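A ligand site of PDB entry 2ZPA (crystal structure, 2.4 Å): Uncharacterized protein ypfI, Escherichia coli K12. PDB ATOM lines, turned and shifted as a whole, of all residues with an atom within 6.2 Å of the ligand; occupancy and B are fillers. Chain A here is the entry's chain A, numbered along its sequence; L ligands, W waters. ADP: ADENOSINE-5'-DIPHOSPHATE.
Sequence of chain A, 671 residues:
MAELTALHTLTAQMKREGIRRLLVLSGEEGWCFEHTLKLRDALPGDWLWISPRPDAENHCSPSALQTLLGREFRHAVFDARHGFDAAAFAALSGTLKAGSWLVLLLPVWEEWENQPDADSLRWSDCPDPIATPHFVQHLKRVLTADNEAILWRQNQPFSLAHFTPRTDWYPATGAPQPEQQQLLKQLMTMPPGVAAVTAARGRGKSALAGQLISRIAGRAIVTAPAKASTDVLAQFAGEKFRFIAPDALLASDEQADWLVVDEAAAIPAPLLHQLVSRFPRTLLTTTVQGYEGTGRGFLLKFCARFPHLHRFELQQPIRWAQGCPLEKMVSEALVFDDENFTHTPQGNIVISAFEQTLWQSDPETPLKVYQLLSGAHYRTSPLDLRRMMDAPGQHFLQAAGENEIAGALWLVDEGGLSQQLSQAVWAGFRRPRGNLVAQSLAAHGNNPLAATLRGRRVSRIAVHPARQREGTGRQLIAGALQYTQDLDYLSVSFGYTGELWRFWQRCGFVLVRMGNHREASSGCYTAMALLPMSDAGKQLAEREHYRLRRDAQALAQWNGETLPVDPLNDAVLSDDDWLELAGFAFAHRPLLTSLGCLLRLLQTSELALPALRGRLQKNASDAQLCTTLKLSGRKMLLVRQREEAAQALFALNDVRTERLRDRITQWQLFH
N of Gly 202 is in hydrogen-bond range of O3B of the ligand (3.1 Å).
The side-chain hydroxyl (OG) of Ser 206 lies within hydrogen-bond range of an oxygen (O1B) of the ligand.
O3A of the ligand sits at hydrogen-bond distance from N of Gly 204 (2.7 Å).
The side-chain amino group (NZ) of Lys 205 lies within salt-bridge range of an oxygen (O3B) of the ligand.
A nitrogen (N6) of the ligand sits at hydrogen-bond distance from the side-chain amide oxygen (OE1) of Gln 180 (2.8 Å).
O3' of the ligand lies close to NE of Arg 319 (3.0 Å).
A nitrogen (N1) of the ligand lies close to the backbone NH (N) of Gly 174.
An oxygen (O1A) of the ligand sits at hydrogen-bond distance from the backbone NH (N) of Ala 207.
N of Arg 203 lies within hydrogen-bond range of O3B of the ligand, at 3.1 Å.
N6 of the ligand is in hydrogen-bond range of O of Ala 175, 3.1 Å away.
O1B of the ligand is in hydrogen-bond range of N of Ser 206 (3.0 Å).
N of Lys 205 is in hydrogen-bond range of O1B of the ligand, at 3.2 Å.
The side-chain amide nitrogen (NE2) of Gln 211 sits close to a nitrogen (N6) of the ligand (3.2 Å).
N of Gln 177 lies within hydrogen-bond range of OE1 of Gln 180, at 3.0 Å.
The backbone carbonyl oxygen (O) of Gly 204 lies within hydrogen-bond range of the side-chain amide nitrogen (NE2) of Gln 180, 3.1 Å away.
OE2 of Glu 72 is in salt-bridge range of NH1 of Arg 319 (3.2 Å).
N of Ile 318 sits at hydrogen-bond distance from O of Gly 202, at 3.0 Å.
NZ of Lys 205 sits at hydrogen-bond distance from O of Ala 199 (3.1 Å).
NE2 of Gln 211 is in hydrogen-bond range of OE1 of Gln 180 (3.1 Å).
O of Arg 201 sits at hydrogen-bond distance from NH1 of Arg 203 (2.9 Å).
The side-chain amino group of Lys 205 lies within hydrogen-bond range of the backbone carbonyl oxygen of Ala 200 (3.3 Å).
Water W1 lies within hydrogen-bond range of an oxygen (O2A) of the ligand (2.6 Å) and the side-chain hydroxyl (OG) of Ser 206 (3.1 Å).
Water W4 bridges an oxygen (O2B) of the ligand (2.7 Å) and the side-chain hydroxyl (OG) of Ser 206 (3.4 Å).
CB of Ala 172 touches N1 of the ligand, 3.5 Å away.
Thr 173 touches the ligand (C to C2, 3.98 Å).
CA of Pro 176 touches N6 of the ligand, at 3.7 Å.
Gln 177 touches the ligand.
Ala 200 touches the ligand (O to O3B, 3.6 Å).
Arg 201 touches the ligand.
Val 232 touches the ligand (CG1 to O2', 3.5 Å).
Phe 236 touches the ligand.
Ile 318 touches the ligand.
Of the 28 residues printed, 20 come within 4 Å of the ligand.
The nearest printed residue that does not touch the ligand is Gln 235 (4.3 Å).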
ATOM      1  N   GLY A  70      -6.995 -37.345  16.468  1.00  0.00           N
ATOM      2  CA  GLY A  70      -7.512 -36.041  16.709  1.00  0.00           C
ATOM      3  C   GLY A  70      -9.036 -36.146  16.687  1.00  0.00           C
ATOM      4  O   GLY A  70      -9.701 -35.160  16.452  1.00  0.00           O
ATOM      5  N   GLU A  72     -12.904 -36.272  17.508  1.00  0.00           N
ATOM      6  CA  GLU A  72     -13.905 -35.739  18.423  1.00  0.00           C
ATOM      7  C   GLU A  72     -15.216 -36.446  18.073  1.00  0.00           C
ATOM      8  O   GLU A  72     -15.445 -36.787  16.908  1.00  0.00           O
ATOM      9  CB  GLU A  72     -14.059 -34.236  18.205  1.00  0.00           C
ATOM     10  CG  GLU A  72     -13.177 -33.699  17.095  1.00  0.00           C
ATOM     11  CD  GLU A  72     -13.586 -32.310  16.619  1.00  0.00           C
ATOM     12  OE1 GLU A  72     -13.335 -32.008  15.420  1.00  0.00           O
ATOM     13  OE2 GLU A  72     -14.150 -31.525  17.413  1.00  0.00           O
ATOM     14  N   ALA A 172     -13.740 -22.531  18.792  1.00  0.00           N
ATOM     15  CA  ALA A 172     -12.571 -21.893  18.235  1.00  0.00           C
ATOM     16  C   ALA A 172     -12.587 -22.111  16.738  1.00  0.00           C
ATOM     17  O   ALA A 172     -12.926 -23.181  16.246  1.00  0.00           O
ATOM     18  CB  ALA A 172     -11.312 -22.485  18.855  1.00  0.00           C
ATOM     19  N   THR A 173     -12.193 -21.062  16.013  1.00  0.00           N
ATOM     20  CA  THR A 173     -12.175 -21.072  14.553  1.00  0.00           C
ATOM     21  C   THR A 173     -10.888 -21.662  14.004  1.00  0.00           C
ATOM     22  O   THR A 173     -10.909 -22.487  13.090  1.00  0.00           O
ATOM     23  CB  THR A 173     -12.298 -19.629  14.036  1.00  0.00           C
ATOM     24  OG1 THR A 173     -10.991 -19.043  13.969  1.00  0.00           O
ATOM     25  CG2 THR A 173     -13.129 -18.801  15.006  1.00  0.00           C
ATOM     26  N   GLY A 174      -9.762 -21.221  14.569  1.00  0.00           N
ATOM     27  CA  GLY A 174      -8.463 -21.683  14.123  1.00  0.00           C
ATOM     28  C   GLY A 174      -7.476 -20.596  14.499  1.00  0.00           C
ATOM     29  O   GLY A 174      -6.282 -20.850  14.629  1.00  0.00           O
ATOM     30  N   ALA A 175      -7.989 -19.384  14.652  1.00  0.00           N
ATOM     31  CA  ALA A 175      -7.172 -18.255  15.045  1.00  0.00           C
ATOM     32  C   ALA A 175      -6.821 -18.498  16.504  1.00  0.00           C
ATOM     33  O   ALA A 175      -7.645 -19.007  17.260  1.00  0.00           O
ATOM     34  CB  ALA A 175      -7.957 -16.963  14.904  1.00  0.00           C
ATOM     35  N   PRO A 176      -5.592 -18.164  16.924  1.00  0.00           N
ATOM     36  CA  PRO A 176      -5.316 -18.418  18.334  1.00  0.00           C
ATOM     37  C   PRO A 176      -6.292 -17.738  19.282  1.00  0.00           C
ATOM     38  O   PRO A 176      -6.633 -16.575  19.106  1.00  0.00           O
ATOM     39  CB  PRO A 176      -3.874 -17.929  18.498  1.00  0.00           C
ATOM     40  CG  PRO A 176      -3.604 -17.085  17.275  1.00  0.00           C
ATOM     41  CD  PRO A 176      -4.371 -17.770  16.203  1.00  0.00           C
ATOM     42  N   GLN A 177      -6.743 -18.486  20.283  1.00  0.00           N
ATOM     43  CA  GLN A 177      -7.658 -17.955  21.287  1.00  0.00           C
ATOM     44  C   GLN A 177      -6.912 -16.905  22.112  1.00  0.00           C
ATOM     45  O   GLN A 177      -5.686 -16.816  22.060  1.00  0.00           O
ATOM     46  CB  GLN A 177      -8.173 -19.086  22.182  1.00  0.00           C
ATOM     47  CG  GLN A 177      -9.139 -20.025  21.468  1.00  0.00           C
ATOM     48  CD  GLN A 177     -10.491 -19.367  21.182  1.00  0.00           C
ATOM     49  OE1 GLN A 177     -11.229 -19.015  22.108  1.00  0.00           O
ATOM     50  NE2 GLN A 177     -10.807 -19.194  19.909  1.00  0.00           N
ATOM     51  N   GLN A 180      -3.857 -17.928  24.038  1.00  0.00           N
ATOM     52  CA  GLN A 180      -2.810 -18.362  23.135  1.00  0.00           C
ATOM     53  C   GLN A 180      -2.151 -17.138  22.508  1.00  0.00           C
ATOM     54  O   GLN A 180      -0.926 -17.011  22.519  1.00  0.00           O
ATOM     55  CB  GLN A 180      -3.383 -19.256  22.032  1.00  0.00           C
ATOM     56  CG  GLN A 180      -4.148 -20.474  22.542  1.00  0.00           C
ATOM     57  CD  GLN A 180      -4.564 -21.405  21.416  1.00  0.00           C
ATOM     58  OE1 GLN A 180      -5.161 -20.973  20.438  1.00  0.00           O
ATOM     59  NE2 GLN A 180      -4.253 -22.698  21.552  1.00  0.00           N
ATOM     60  N   ALA A 199       0.194 -26.884  31.282  1.00  0.00           N
ATOM     61  CA  ALA A 199      -1.270 -26.829  31.320  1.00  0.00           C
ATOM     62  C   ALA A 199      -1.956 -28.186  31.332  1.00  0.00           C
ATOM     63  O   ALA A 199      -1.390 -29.190  30.905  1.00  0.00           O
ATOM     64  CB  ALA A 199      -1.788 -26.022  30.118  1.00  0.00           C
ATOM     65  N   ALA A 200      -3.200 -28.188  31.818  1.00  0.00           N
ATOM     66  CA  ALA A 200      -4.031 -29.396  31.839  1.00  0.00           C
ATOM     67  C   ALA A 200      -4.283 -29.770  30.375  1.00  0.00           C
ATOM     68  O   ALA A 200      -4.169 -28.916  29.488  1.00  0.00           O
ATOM     69  CB  ALA A 200      -5.349 -29.105  32.512  1.00  0.00           C
ATOM     70  N   ARG A 201      -4.613 -31.030  30.123  1.00  0.00           N
ATOM     71  CA  ARG A 201      -4.868 -31.486  28.761  1.00  0.00           C
ATOM     72  C   ARG A 201      -6.042 -30.701  28.154  1.00  0.00           C
ATOM     73  O   ARG A 201      -6.965 -30.298  28.861  1.00  0.00           O
ATOM     74  CB  ARG A 201      -5.161 -32.989  28.763  1.00  0.00           C
ATOM     75  CG  ARG A 201      -5.757 -33.504  27.451  1.00  0.00           C
ATOM     76  CD  ARG A 201      -5.698 -35.019  27.365  1.00  0.00           C
ATOM     77  NE  ARG A 201      -4.364 -35.510  27.710  1.00  0.00           N
ATOM     78  CZ  ARG A 201      -3.318 -36.172  27.231  1.00  0.00           C
ATOM     79  NH1 ARG A 201      -3.149 -36.319  25.922  1.00  0.00           N
ATOM     80  NH2 ARG A 201      -2.413 -36.678  28.065  1.00  0.00           N
ATOM     81  N   GLY A 202      -5.988 -30.492  26.836  1.00  0.00           N
ATOM     82  CA  GLY A 202      -7.048 -29.774  26.140  1.00  0.00           C
ATOM     83  C   GLY A 202      -7.029 -28.251  26.265  1.00  0.00           C
ATOM     84  O   GLY A 202      -8.063 -27.603  26.056  1.00  0.00           O
ATOM     85  N   ARG A 203      -5.886 -27.669  26.613  1.00  0.00           N
ATOM     86  CA  ARG A 203      -5.782 -26.222  26.732  1.00  0.00           C
ATOM     87  C   ARG A 203      -5.108 -25.563  25.537  1.00  0.00           C
ATOM     88  O   ARG A 203      -4.838 -24.369  25.546  1.00  0.00           O
ATOM     89  CB  ARG A 203      -5.042 -25.846  28.010  1.00  0.00           C
ATOM     90  CG  ARG A 203      -5.950 -25.681  29.214  1.00  0.00           C
ATOM     91  CD  ARG A 203      -6.811 -26.934  29.503  1.00  0.00           C
ATOM     92  NE  ARG A 203      -7.717 -26.690  30.628  1.00  0.00           N
ATOM     93  CZ  ARG A 203      -8.658 -27.530  31.040  1.00  0.00           C
ATOM     94  NH1 ARG A 203      -8.833 -28.702  30.419  1.00  0.00           N
ATOM     95  NH2 ARG A 203      -9.452 -27.204  32.058  1.00  0.00           N
ATOM     96  N   GLY A 204      -4.811 -26.363  24.514  1.00  0.00           N
ATOM     97  CA  GLY A 204      -4.198 -25.801  23.324  1.00  0.00           C
ATOM     98  C   GLY A 204      -2.691 -25.591  23.339  1.00  0.00           C
ATOM     99  O   GLY A 204      -2.190 -24.714  22.634  1.00  0.00           O
ATOM    100  N   LYS A 205      -1.971 -26.384  24.122  1.00  0.00           N
ATOM    101  CA  LYS A 205      -0.516 -26.258  24.194  1.00  0.00           C
ATOM    102  C   LYS A 205       0.133 -26.655  22.857  1.00  0.00           C
ATOM    103  O   LYS A 205       0.979 -25.925  22.337  1.00  0.00           O
ATOM    104  CB  LYS A 205       0.053 -27.139  25.315  1.00  0.00           C
ATOM    105  CG  LYS A 205      -0.424 -26.767  26.728  1.00  0.00           C
ATOM    106  CD  LYS A 205       0.275 -27.609  27.815  1.00  0.00           C
ATOM    107  CE  LYS A 205       0.029 -29.111  27.623  1.00  0.00           C
ATOM    108  NZ  LYS A 205      -1.387 -29.521  27.841  1.00  0.00           N
ATOM    109  N   SER A 206      -0.243 -27.812  22.319  1.00  0.00           N
ATOM    110  CA  SER A 206       0.347 -28.277  21.054  1.00  0.00           C
ATOM    111  C   SER A 206       0.008 -27.335  19.898  1.00  0.00           C
ATOM    112  O   SER A 206       0.817 -27.129  19.000  1.00  0.00           O
ATOM    113  CB  SER A 206      -0.141 -29.696  20.737  1.00  0.00           C
ATOM    114  OG  SER A 206       0.193 -30.611  21.774  1.00  0.00           O
ATOM    115  N   ALA A 207      -1.199 -26.765  19.909  1.00  0.00           N
ATOM    116  CA  ALA A 207      -1.611 -25.842  18.870  1.00  0.00           C
ATOM    117  C   ALA A 207      -0.794 -24.543  19.021  1.00  0.00           C
ATOM    118  O   ALA A 207      -0.357 -23.963  18.040  1.00  0.00           O
ATOM    119  CB  ALA A 207      -3.099 -25.558  18.988  1.00  0.00           C
ATOM    120  N   LEU A 208      -0.613 -24.106  20.261  1.00  0.00           N
ATOM    121  CA  LEU A 208       0.178 -22.913  20.505  1.00  0.00           C
ATOM    122  C   LEU A 208       1.570 -23.095  19.925  1.00  0.00           C
ATOM    123  O   LEU A 208       2.127 -22.176  19.329  1.00  0.00           O
ATOM    124  CB  LEU A 208       0.315 -22.651  22.009  1.00  0.00           C
ATOM    125  CG  LEU A 208       1.318 -21.583  22.407  1.00  0.00           C
ATOM    126  CD1 LEU A 208       0.886 -20.222  21.858  1.00  0.00           C
ATOM    127  CD2 LEU A 208       1.418 -21.529  23.906  1.00  0.00           C
ATOM    128  N   GLN A 211       1.230 -22.883  16.239  1.00  0.00           N
ATOM    129  CA  GLN A 211       0.907 -21.542  15.824  1.00  0.00           C
ATOM    130  C   GLN A 211       2.186 -20.724  15.846  1.00  0.00           C
ATOM    131  O   GLN A 211       2.378 -19.821  15.039  1.00  0.00           O
ATOM    132  CB  GLN A 211      -0.129 -20.929  16.768  1.00  0.00           C
ATOM    133  CG  GLN A 211      -1.455 -21.680  16.809  1.00  0.00           C
ATOM    134  CD  GLN A 211      -2.378 -21.154  17.888  1.00  0.00           C
ATOM    135  OE1 GLN A 211      -1.938 -20.538  18.865  1.00  0.00           O
ATOM    136  NE2 GLN A 211      -3.685 -21.406  17.724  1.00  0.00           N
ATOM    137  N   VAL A 232      -1.798 -32.510  16.053  1.00  0.00           N
ATOM    138  CA  VAL A 232      -2.383 -31.187  16.258  1.00  0.00           C
ATOM    139  C   VAL A 232      -1.309 -30.122  16.056  1.00  0.00           C
ATOM    140  O   VAL A 232      -1.561 -29.072  15.463  1.00  0.00           O
ATOM    141  CB  VAL A 232      -2.982 -31.027  17.667  1.00  0.00           C
ATOM    142  CG1 VAL A 232      -3.387 -29.584  17.880  1.00  0.00           C
ATOM    143  CG2 VAL A 232      -4.168 -31.960  17.838  1.00  0.00           C
ATOM    144  N   LEU A 233      -0.107 -30.407  16.536  1.00  0.00           N
ATOM    145  CA  LEU A 233       0.997 -29.472  16.407  1.00  0.00           C
ATOM    146  C   LEU A 233       1.323 -29.266  14.924  1.00  0.00           C
ATOM    147  O   LEU A 233       1.498 -28.139  14.473  1.00  0.00           O
ATOM    148  CB  LEU A 233       2.213 -29.979  17.183  1.00  0.00           C
ATOM    149  CG  LEU A 233       3.266 -28.930  17.578  1.00  0.00           C
ATOM    150  CD1 LEU A 233       4.297 -29.550  18.527  1.00  0.00           C
ATOM    151  CD2 LEU A 233       3.942 -28.371  16.331  1.00  0.00           C
ATOM    152  N   GLN A 235      -0.642 -29.743  12.354  1.00  0.00           N
ATOM    153  CA  GLN A 235      -1.762 -29.061  11.730  1.00  0.00           C
ATOM    154  C   GLN A 235      -1.602 -27.543  11.786  1.00  0.00           C
ATOM    155  O   GLN A 235      -1.818 -26.859  10.781  1.00  0.00           O
ATOM    156  CB  GLN A 235      -3.078 -29.451  12.425  1.00  0.00           C
ATOM    157  CG  GLN A 235      -4.319 -28.744  11.902  1.00  0.00           C
ATOM    158  CD  GLN A 235      -5.526 -28.906  12.811  1.00  0.00           C
ATOM    159  OE1 GLN A 235      -5.791 -30.010  13.306  1.00  0.00           O
ATOM    160  NE2 GLN A 235      -6.266 -27.830  13.036  1.00  0.00           N
ATOM    161  N   PHE A 236      -1.231 -27.009  12.945  1.00  0.00           N
ATOM    162  CA  PHE A 236      -1.067 -25.552  13.066  1.00  0.00           C
ATOM    163  C   PHE A 236       0.271 -25.073  12.510  1.00  0.00           C
ATOM    164  O   PHE A 236       0.438 -23.894  12.213  1.00  0.00           O
ATOM    165  CB  PHE A 236      -1.236 -25.095  14.521  1.00  0.00           C
ATOM    166  CG  PHE A 236      -2.648 -25.229  15.039  1.00  0.00           C
ATOM    167  CD1 PHE A 236      -3.117 -26.464  15.492  1.00  0.00           C
ATOM    168  CD2 PHE A 236      -3.522 -24.142  15.019  1.00  0.00           C
ATOM    169  CE1 PHE A 236      -4.450 -26.608  15.926  1.00  0.00           C
ATOM    170  CE2 PHE A 236      -4.848 -24.273  15.450  1.00  0.00           C
ATOM    171  CZ  PHE A 236      -5.315 -25.511  15.894  1.00  0.00           C
ATOM    172  N   GLU A 263       5.715 -32.223  25.532  1.00  0.00           N
ATOM    173  CA  GLU A 263       5.786 -33.341  26.458  1.00  0.00           C
ATOM    174  C   GLU A 263       7.268 -33.536  26.689  1.00  0.00           C
ATOM    175  O   GLU A 263       7.793 -34.645  26.635  1.00  0.00           O
ATOM    176  CB  GLU A 263       5.156 -34.605  25.867  1.00  0.00           C
ATOM    177  CG  GLU A 263       3.649 -34.517  25.644  1.00  0.00           C
ATOM    178  CD  GLU A 263       2.900 -33.885  26.810  1.00  0.00           C
ATOM    179  OE1 GLU A 263       3.126 -34.260  27.975  1.00  0.00           O
ATOM    180  OE2 GLU A 263       2.062 -33.000  26.552  1.00  0.00           O
ATOM    181  N   THR A 287       1.772 -31.503  29.595  1.00  0.00           N
ATOM    182  CA  THR A 287       0.460 -31.454  30.198  1.00  0.00           C
ATOM    183  C   THR A 287       0.622 -31.850  31.657  1.00  0.00           C
ATOM    184  O   THR A 287       1.451 -32.688  32.006  1.00  0.00           O
ATOM    185  CB  THR A 287      -0.547 -32.377  29.501  1.00  0.00           C
ATOM    186  OG1 THR A 287      -0.491 -33.675  30.092  1.00  0.00           O
ATOM    187  CG2 THR A 287      -0.222 -32.476  28.021  1.00  0.00           C
ATOM    188  N   ILE A 318     -10.056 -25.421  25.340  1.00  0.00           N
ATOM    189  CA  ILE A 318     -10.476 -24.892  24.050  1.00  0.00           C
ATOM    190  C   ILE A 318     -11.695 -25.495  23.363  1.00  0.00           C
ATOM    191  O   ILE A 318     -12.376 -24.808  22.593  1.00  0.00           O
ATOM    192  CB  ILE A 318      -9.278 -24.893  23.030  1.00  0.00           C
ATOM    193  CG1 ILE A 318      -9.555 -25.832  21.858  1.00  0.00           C
ATOM    194  CG2 ILE A 318      -7.988 -25.258  23.735  1.00  0.00           C
ATOM    195  CD1 ILE A 318     -10.242 -25.152  20.675  1.00  0.00           C
ATOM    196  N   ARG A 319     -11.991 -26.769  23.614  1.00  0.00           N
ATOM    197  CA  ARG A 319     -13.142 -27.403  22.988  1.00  0.00           C
ATOM    198  C   ARG A 319     -14.407 -27.455  23.855  1.00  0.00           C
ATOM    199  O   ARG A 319     -15.407 -28.059  23.476  1.00  0.00           O
ATOM    200  CB  ARG A 319     -12.762 -28.788  22.476  1.00  0.00           C
ATOM    201  CG  ARG A 319     -11.870 -28.681  21.252  1.00  0.00           C
ATOM    202  CD  ARG A 319     -11.705 -29.993  20.518  1.00  0.00           C
ATOM    203  NE  ARG A 319     -11.291 -29.770  19.139  1.00  0.00           N
ATOM    204  CZ  ARG A 319     -11.098 -30.739  18.254  1.00  0.00           C
ATOM    205  NH1 ARG A 319     -11.268 -32.010  18.602  1.00  0.00           N
ATOM    206  NH2 ARG A 319     -10.704 -30.429  17.014  1.00  0.00           N
HETATM  207  PB  ADP L   1      -3.262 -29.799  24.598  1.00  0.00           P
HETATM  208  O1B ADP L   1      -1.926 -29.567  24.048  1.00  0.00           O
HETATM  209  O2B ADP L   1      -3.653 -31.340  24.641  1.00  0.00           O
HETATM  210  O3B ADP L   1      -3.275 -29.187  26.054  1.00  0.00           O
HETATM  211  PA  ADP L   1      -4.267 -29.240  22.197  1.00  0.00           P
HETATM  212  O1A ADP L   1      -3.763 -27.979  21.647  1.00  0.00           O
HETATM  213  O2A ADP L   1      -3.156 -30.245  21.665  1.00  0.00           O
HETATM  214  O3A ADP L   1      -4.371 -28.937  23.775  1.00  0.00           O
HETATM  215  O5' ADP L   1      -5.599 -29.511  21.390  1.00  0.00           O
HETATM  216  C5' ADP L   1      -6.749 -28.845  21.906  1.00  0.00           C
HETATM  217  C4' ADP L   1      -7.880 -29.109  20.878  1.00  0.00           C
HETATM  218  O4' ADP L   1      -8.491 -27.930  20.332  1.00  0.00           O
HETATM  219  C3' ADP L   1      -7.393 -29.944  19.678  1.00  0.00           C
HETATM  220  O3' ADP L   1      -8.466 -30.687  19.109  1.00  0.00           O
HETATM  221  C2' ADP L   1      -6.868 -28.801  18.749  1.00  0.00           C
HETATM  222  O2' ADP L   1      -6.833 -29.165  17.379  1.00  0.00           O
HETATM  223  C1' ADP L   1      -7.954 -27.705  18.996  1.00  0.00           C
HETATM  224  N9  ADP L   1      -7.477 -26.323  19.018  1.00  0.00           N
HETATM  225  C8  ADP L   1      -6.533 -25.785  19.849  1.00  0.00           C
HETATM  226  N7  ADP L   1      -6.373 -24.527  19.612  1.00  0.00           N
HETATM  227  C5  ADP L   1      -7.189 -24.159  18.597  1.00  0.00           C
HETATM  228  C6  ADP L   1      -7.455 -22.957  17.917  1.00  0.00           C
HETATM  229  N6  ADP L   1      -6.775 -21.798  18.274  1.00  0.00           N
HETATM  230  N1  ADP L   1      -8.373 -22.951  16.932  1.00  0.00           N
HETATM  231  C2  ADP L   1      -9.033 -24.055  16.583  1.00  0.00           C
HETATM  232  N3  ADP L   1      -8.823 -25.225  17.194  1.00  0.00           N
HETATM  233  C4  ADP L   1      -7.919 -25.316  18.204  1.00  0.00           C
HETATM  234  O   HOH W   1      -2.136 -32.626  21.114  1.00  0.00           O
HETATM  235  O   HOH W   2      -5.620 -32.440  23.552  1.00  0.00           O
HETATM  236  O   HOH W   3     -10.707 -25.252  13.853  1.00  0.00           O
HETATM  237  O   HOH W   4      -1.401 -32.669  24.032  1.00  0.00           O
